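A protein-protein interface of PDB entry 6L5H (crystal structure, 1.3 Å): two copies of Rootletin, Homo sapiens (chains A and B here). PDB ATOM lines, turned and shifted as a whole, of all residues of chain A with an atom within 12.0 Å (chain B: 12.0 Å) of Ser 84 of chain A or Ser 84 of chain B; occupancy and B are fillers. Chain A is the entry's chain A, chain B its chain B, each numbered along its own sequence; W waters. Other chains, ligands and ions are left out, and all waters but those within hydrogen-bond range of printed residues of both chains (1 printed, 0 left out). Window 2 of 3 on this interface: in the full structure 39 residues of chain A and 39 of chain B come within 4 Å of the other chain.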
ATOM      1  N   LEU A  75      -7.212 -17.007  30.763  1.00  0.00           N
ATOM      2  CA  LEU A  75      -7.492 -15.819  29.963  1.00  0.00           C
ATOM      3  C   LEU A  75      -7.289 -16.098  28.476  1.00  0.00           C
ATOM      4  O   LEU A  75      -8.094 -15.672  27.632  1.00  0.00           O
ATOM      5  CB  LEU A  75      -6.593 -14.675  30.421  1.00  0.00           C
ATOM      6  CG  LEU A  75      -6.693 -13.320  29.737  1.00  0.00           C
ATOM      7  CD1 LEU A  75      -7.949 -12.615  30.220  1.00  0.00           C
ATOM      8  CD2 LEU A  75      -5.435 -12.496  30.016  1.00  0.00           C
ATOM      9  N   GLU A  76      -6.228 -16.832  28.142  1.00  0.00           N
ATOM     10  CA  GLU A  76      -5.926 -17.118  26.741  1.00  0.00           C
ATOM     11  C   GLU A  76      -6.950 -18.070  26.116  1.00  0.00           C
ATOM     12  O   GLU A  76      -7.329 -17.906  24.945  1.00  0.00           O
ATOM     13  CB  GLU A  76      -4.502 -17.678  26.640  1.00  0.00           C
ATOM     14  CG  GLU A  76      -4.087 -18.209  25.277  1.00  0.00           C
ATOM     15  CD  GLU A  76      -4.177 -17.177  24.165  1.00  0.00           C
ATOM     16  OE1 GLU A  76      -4.258 -15.962  24.449  1.00  0.00           O
ATOM     17  OE2 GLU A  76      -4.155 -17.593  22.989  1.00  0.00           O
ATOM     18  N   ALA A  77      -7.401 -19.075  26.869  1.00  0.00           N
ATOM     19  CA  ALA A  77      -8.432 -19.981  26.366  1.00  0.00           C
ATOM     20  C   ALA A  77      -9.745 -19.236  26.125  1.00  0.00           C
ATOM     21  O   ALA A  77     -10.445 -19.489  25.124  1.00  0.00           O
ATOM     22  CB  ALA A  77      -8.628 -21.131  27.357  1.00  0.00           C
ATOM     23  N   GLN A  78     -10.081 -18.289  27.010  1.00  0.00           N
ATOM     24  CA  GLN A  78     -11.256 -17.444  26.781  1.00  0.00           C
ATOM     25  C   GLN A  78     -11.098 -16.600  25.521  1.00  0.00           C
ATOM     26  O   GLN A  78     -12.070 -16.380  24.776  1.00  0.00           O
ATOM     27  CB  GLN A  78     -11.491 -16.530  27.982  1.00  0.00           C
ATOM     28  CG  GLN A  78     -11.935 -17.259  29.212  1.00  0.00           C
ATOM     29  CD  GLN A  78     -11.970 -16.347  30.412  1.00  0.00           C
ATOM     30  OE1 GLN A  78     -11.360 -15.276  30.405  1.00  0.00           O
ATOM     31  NE2 GLN A  78     -12.694 -16.753  31.441  1.00  0.00           N
ATOM     32  N   ARG A  79      -9.887 -16.084  25.297  1.00  0.00           N
ATOM     33  CA  ARG A  79      -9.628 -15.277  24.111  1.00  0.00           C
ATOM     34  C   ARG A  79      -9.794 -16.110  22.848  1.00  0.00           C
ATOM     35  O   ARG A  79     -10.411 -15.664  21.869  1.00  0.00           O
ATOM     36  CB  ARG A  79      -8.221 -14.671  24.181  1.00  0.00           C
ATOM     37  CG  ARG A  79      -7.921 -13.685  23.046  1.00  0.00           C
ATOM     38  CD  ARG A  79      -6.416 -13.459  22.856  1.00  0.00           C
ATOM     39  NE  ARG A  79      -5.744 -14.679  22.404  1.00  0.00           N
ATOM     40  CZ  ARG A  79      -5.758 -15.115  21.147  1.00  0.00           C
ATOM     41  NH1 ARG A  79      -6.404 -14.431  20.215  1.00  0.00           N
ATOM     42  NH2 ARG A  79      -5.130 -16.237  20.820  1.00  0.00           N
ATOM     43  N   LYS A  80      -9.261 -17.336  22.860  1.00  0.00           N
ATOM     44  CA  LYS A  80      -9.395 -18.214  21.698  1.00  0.00           C
ATOM     45  C   LYS A  80     -10.860 -18.517  21.407  1.00  0.00           C
ATOM     46  O   LYS A  80     -11.265 -18.620  20.240  1.00  0.00           O
ATOM     47  CB  LYS A  80      -8.623 -19.518  21.925  1.00  0.00           C
ATOM     48  CG  LYS A  80      -7.115 -19.389  21.942  1.00  0.00           C
ATOM     49  CD  LYS A  80      -6.470 -20.769  22.141  1.00  0.00           C
ATOM     50  CE  LYS A  80      -5.160 -20.689  22.941  1.00  0.00           C
ATOM     51  NZ  LYS A  80      -5.086 -21.555  24.186  1.00  0.00           N
ATOM     52  N   LEU A  81     -11.670 -18.678  22.454  1.00  0.00           N
ATOM     53  CA  LEU A  81     -13.083 -18.962  22.236  1.00  0.00           C
ATOM     54  C   LEU A  81     -13.798 -17.770  21.604  1.00  0.00           C
ATOM     55  O   LEU A  81     -14.695 -17.949  20.757  1.00  0.00           O
ATOM     56  CB  LEU A  81     -13.749 -19.338  23.560  1.00  0.00           C
ATOM     57  CG  LEU A  81     -15.155 -19.917  23.401  1.00  0.00           C
ATOM     58  CD1 LEU A  81     -15.117 -21.228  22.624  1.00  0.00           C
ATOM     59  CD2 LEU A  81     -15.780 -20.115  24.776  1.00  0.00           C
ATOM     60  N   ARG A  82     -13.385 -16.556  21.965  1.00  0.00           N
ATOM     61  CA  ARG A  82     -13.976 -15.380  21.336  1.00  0.00           C
ATOM     62  C   ARG A  82     -13.595 -15.260  19.867  1.00  0.00           C
ATOM     63  O   ARG A  82     -14.385 -14.737  19.070  1.00  0.00           O
ATOM     64  CB  ARG A  82     -13.571 -14.128  22.097  1.00  0.00           C
ATOM     65  CG  ARG A  82     -14.362 -13.921  23.364  1.00  0.00           C
ATOM     66  CD  ARG A  82     -13.797 -12.743  24.131  1.00  0.00           C
ATOM     67  NE  ARG A  82     -14.623 -12.380  25.276  1.00  0.00           N
ATOM     68  CZ  ARG A  82     -15.671 -11.563  25.218  1.00  0.00           C
ATOM     69  NH1 ARG A  82     -16.047 -11.015  24.057  1.00  0.00           N
ATOM     70  NH2 ARG A  82     -16.345 -11.297  26.326  1.00  0.00           N
ATOM     71  N   GLU A  83     -12.406 -15.724  19.487  1.00  0.00           N
ATOM     72  CA  GLU A  83     -11.955 -15.658  18.099  1.00  0.00           C
ATOM     73  C   GLU A  83     -12.402 -16.859  17.277  1.00  0.00           C
ATOM     74  O   GLU A  83     -12.247 -16.849  16.048  1.00  0.00           O
ATOM     75  CB  GLU A  83     -10.424 -15.536  18.048  1.00  0.00           C
ATOM     76  CG  GLU A  83      -9.848 -15.136  16.690  1.00  0.00           C
ATOM     77  CD  GLU A  83     -10.168 -13.700  16.311  1.00  0.00           C
ATOM     78  OE1 GLU A  83     -10.127 -12.828  17.207  1.00  0.00           O
ATOM     79  OE2 GLU A  83     -10.464 -13.447  15.121  1.00  0.00           O
ATOM     80  N   SER A  84     -12.957 -17.882  17.918  1.00  0.00           N
ATOM     81  CA  SER A  84     -13.408 -19.088  17.242  1.00  0.00           C
ATOM     82  C   SER A  84     -14.693 -18.832  16.458  1.00  0.00           C
ATOM     83  O   SER A  84     -14.725 -18.972  15.235  1.00  0.00           O
ATOM     84  CB  SER A  84     -13.620 -20.210  18.262  1.00  0.00           C
ATOM     85  OG  SER A  84     -14.081 -21.395  17.640  1.00  0.00           O
ATOM     86  N   LEU B  75      -9.653 -26.099  32.646  1.00  0.00           N
ATOM     87  CA  LEU B  75     -10.117 -27.322  31.996  1.00  0.00           C
ATOM     88  C   LEU B  75     -11.513 -27.129  31.384  1.00  0.00           C
ATOM     89  O   LEU B  75     -11.792 -27.610  30.270  1.00  0.00           O
ATOM     90  CB  LEU B  75     -10.071 -28.487  32.997  1.00  0.00           C
ATOM     91  CG  LEU B  75      -8.636 -28.928  33.346  1.00  0.00           C
ATOM     92  CD1 LEU B  75      -8.583 -29.703  34.649  1.00  0.00           C
ATOM     93  CD2 LEU B  75      -7.985 -29.750  32.224  1.00  0.00           C
ATOM     94  N   GLU B  76     -12.388 -26.383  32.071  1.00  0.00           N
ATOM     95  CA  GLU B  76     -13.712 -26.105  31.505  1.00  0.00           C
ATOM     96  C   GLU B  76     -13.627 -25.229  30.254  1.00  0.00           C
ATOM     97  O   GLU B  76     -14.362 -25.448  29.269  1.00  0.00           O
ATOM     98  CB  GLU B  76     -14.606 -25.428  32.545  1.00  0.00           C
ATOM     99  CG  GLU B  76     -15.348 -26.366  33.477  1.00  0.00           C
ATOM    100  CD  GLU B  76     -16.228 -27.386  32.745  1.00  0.00           C
ATOM    101  OE1 GLU B  76     -16.812 -27.073  31.675  1.00  0.00           O
ATOM    102  OE2 GLU B  76     -16.327 -28.522  33.260  1.00  0.00           O
ATOM    103  N   ALA B  77     -12.770 -24.205  30.283  1.00  0.00           N
ATOM    104  CA  ALA B  77     -12.576 -23.374  29.095  1.00  0.00           C
ATOM    105  C   ALA B  77     -12.049 -24.202  27.928  1.00  0.00           C
ATOM    106  O   ALA B  77     -12.445 -23.998  26.772  1.00  0.00           O
ATOM    107  CB  ALA B  77     -11.618 -22.222  29.411  1.00  0.00           C
ATOM    108  N   GLN B  78     -11.146 -25.141  28.206  1.00  0.00           N
ATOM    109  CA  GLN B  78     -10.641 -25.995  27.136  1.00  0.00           C
ATOM    110  C   GLN B  78     -11.732 -26.910  26.596  1.00  0.00           C
ATOM    111  O   GLN B  78     -11.768 -27.186  25.385  1.00  0.00           O
ATOM    112  CB  GLN B  78      -9.436 -26.799  27.635  1.00  0.00           C
ATOM    113  CG  GLN B  78      -8.192 -25.929  27.816  1.00  0.00           C
ATOM    114  CD  GLN B  78      -7.031 -26.641  28.482  1.00  0.00           C
ATOM    115  OE1 GLN B  78      -7.214 -27.512  29.334  1.00  0.00           O
ATOM    116  NE2 GLN B  78      -5.823 -26.259  28.101  1.00  0.00           N
ATOM    117  N   ARG B  79     -12.642 -27.364  27.460  1.00  0.00           N
ATOM    118  CA  ARG B  79     -13.800 -28.112  26.980  1.00  0.00           C
ATOM    119  C   ARG B  79     -14.600 -27.284  25.985  1.00  0.00           C
ATOM    120  O   ARG B  79     -14.940 -27.760  24.897  1.00  0.00           O
ATOM    121  CB  ARG B  79     -14.689 -28.539  28.151  1.00  0.00           C
ATOM    122  CG  ARG B  79     -15.825 -29.470  27.726  1.00  0.00           C
ATOM    123  CD  ARG B  79     -16.919 -29.560  28.780  1.00  0.00           C
ATOM    124  NE  ARG B  79     -16.390 -29.751  30.130  1.00  0.00           N
ATOM    125  CZ  ARG B  79     -16.029 -30.928  30.637  1.00  0.00           C
ATOM    126  NH1 ARG B  79     -16.128 -32.030  29.905  1.00  0.00           N
ATOM    127  NH2 ARG B  79     -15.567 -31.001  31.877  1.00  0.00           N
ATOM    128  N   LYS B  80     -14.896 -26.028  26.339  1.00  0.00           N
ATOM    129  CA  LYS B  80     -15.664 -25.177  25.426  1.00  0.00           C
ATOM    130  C   LYS B  80     -14.944 -24.988  24.099  1.00  0.00           C
ATOM    131  O   LYS B  80     -15.586 -24.912  23.039  1.00  0.00           O
ATOM    132  CB  LYS B  80     -15.920 -23.810  26.052  1.00  0.00           C
ATOM    133  CG  LYS B  80     -16.962 -23.788  27.127  1.00  0.00           C
ATOM    134  CD  LYS B  80     -17.158 -22.360  27.610  1.00  0.00           C
ATOM    135  CE  LYS B  80     -18.205 -22.286  28.691  1.00  0.00           C
ATOM    136  NZ  LYS B  80     -17.756 -22.917  29.952  1.00  0.00           N
ATOM    137  N   LEU B  81     -13.616 -24.859  24.140  1.00  0.00           N
ATOM    138  CA  LEU B  81     -12.857 -24.732  22.897  1.00  0.00           C
ATOM    139  C   LEU B  81     -13.011 -25.972  22.026  1.00  0.00           C
ATOM    140  O   LEU B  81     -13.146 -25.862  20.800  1.00  0.00           O
ATOM    141  CB  LEU B  81     -11.384 -24.475  23.201  1.00  0.00           C
ATOM    142  CG  LEU B  81     -11.000 -23.005  23.318  1.00  0.00           C
ATOM    143  CD1 LEU B  81      -9.570 -22.862  23.820  1.00  0.00           C
ATOM    144  CD2 LEU B  81     -11.180 -22.293  21.980  1.00  0.00           C
ATOM    145  N   ARG B  82     -13.001 -27.162  22.638  1.00  0.00           N
ATOM    146  CA  ARG B  82     -13.179 -28.383  21.852  1.00  0.00           C
ATOM    147  C   ARG B  82     -14.571 -28.458  21.240  1.00  0.00           C
ATOM    148  O   ARG B  82     -14.718 -28.804  20.064  1.00  0.00           O
ATOM    149  CB  ARG B  82     -12.925 -29.617  22.712  1.00  0.00           C
ATOM    150  CG  ARG B  82     -11.483 -29.826  23.027  1.00  0.00           C
ATOM    151  CD  ARG B  82     -11.267 -31.110  23.778  1.00  0.00           C
ATOM    152  NE  ARG B  82     -10.316 -30.860  24.842  1.00  0.00           N
ATOM    153  CZ  ARG B  82     -10.639 -30.737  26.125  1.00  0.00           C
ATOM    154  NH1 ARG B  82     -11.898 -30.889  26.521  1.00  0.00           N
ATOM    155  NH2 ARG B  82      -9.694 -30.486  27.010  1.00  0.00           N
ATOM    156  N   GLU B  83     -15.607 -28.164  22.027  1.00  0.00           N
ATOM    157  CA  GLU B  83     -16.970 -28.261  21.517  1.00  0.00           C
ATOM    158  C   GLU B  83     -17.264 -27.214  20.449  1.00  0.00           C
ATOM    159  O   GLU B  83     -18.156 -27.430  19.622  1.00  0.00           O
ATOM    160  CB  GLU B  83     -17.990 -28.115  22.652  1.00  0.00           C
ATOM    161  CG  GLU B  83     -17.669 -28.881  23.924  1.00  0.00           C
ATOM    162  CD  GLU B  83     -17.496 -30.369  23.702  1.00  0.00           C
ATOM    163  OE1 GLU B  83     -18.274 -30.952  22.917  1.00  0.00           O
ATOM    164  OE2 GLU B  83     -16.582 -30.953  24.322  1.00  0.00           O
ATOM    165  N   SER B  84     -16.540 -26.099  20.445  1.00  0.00           N
ATOM    166  CA  SER B  84     -16.798 -25.011  19.509  1.00  0.00           C
ATOM    167  C   SER B  84     -16.590 -25.465  18.070  1.00  0.00           C
ATOM    168  O   SER B  84     -17.139 -24.865  17.149  1.00  0.00           O
ATOM    169  CB  SER B  84     -15.898 -23.812  19.813  1.00  0.00           C
ATOM    170  OG  SER B  84     -16.247 -22.700  19.003  1.00  0.00           O
HETATM  171  O   HOH W   1     -12.597 -21.127  26.263  1.00  0.00           O
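The side-chain hydroxyl (OG) of Ser 84 of chain A sits at hydrogen-bond distance from the side-chain hydroxyl (OG) of Ser 84 of chain B, 2.9 Å away.
Printed residues of chain B within 4 Å of Ser 84 of chain A: Ser 84 (2.9 Å).
Of chain A, only Leu 81 and Ser 84 come within 4 Å of Ser 84 of chain B.
No residue of chain B comes within 4 Å of Glu 83 of chain A.
Leu 81 of chain B touches just these residues of chain A: Ala 77, Lys 80 and Leu 81.
No residue of chain A comes within 4 Å of Glu 83 of chain B.
Printed residues of chain A within 4 Å of Ala 77 of chain B: Ala 77.
Of the printed residues of chain A, Lys 80 of chain B touches Leu 81.
Printed residues of chain B within 4 Å of Ala 77 of chain A: Ala 77 (3.8 Å) and Leu 81 (3.7 Å).
Of the printed residues of chain B, Lys 80 of chain A touches Leu 81 (3.8 Å).
Arg 82 of chain A touches none of the printed residues of chain B.
The nearest residue of chain B that does not touch Ser 84 of chain A is Leu 81 of chain B (4.9 Å).
The nearest residue of chain A that does not touch Ser 84 of chain B is Lys 80 of chain A (6.6 Å).
Ala 77 of chain A touches Leu 81 of chain B, but with the chains exchanged Leu 81 of chain A does not touch Ala 77 of chain B (5.5 Å).
Lys 80 of chain A touches Leu 81 of chain B, and with the chains exchanged Leu 81 of chain A touches Lys 80 of chain B.
Leu 81 of chain A touches Ser 84 of chain B, but with the chains exchanged Ser 84 of chain A does not touch Leu 81 of chain B (4.9 Å).
Ser 84 of chain B touches its own counterpart, Ser 84 of chain A.
10 positions are printed for both chains.
Among the printed residues, pairs that only touch across the chains: Leu 81 of chain A with Leu 81 of chain B, Ala 77 of chain A with Leu 81 of chain B, Leu 81 of chain A with Lys 80 of chain B, Lys 80 of chain A with Leu 81 of chain B, Ala 77 of chain A with Ala 77 of chain B and Leu 81 of chain A with Ser 84 of chain B.
Hydrophobic or aromatic side chains of chain B within 4 Å of the printed part of chain A: Ala 77 and Leu 81.
Hydrophobic or aromatic side chains of chain A that line the printed part of chain B: Ala 77 and Leu 81.
Among the printed residues, no Asp or Glu carboxylate lies within 4 Å of a Lys or Arg side-chain nitrogen of the other chain.
Water W1 lies within hydrogen-bond range of the backbone carbonyl oxygen (O) of Ala 77 of chain B (2.9 Å) and the backbone carbonyl oxygen (O) of Ala 77 of chain A (2.9 Å).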
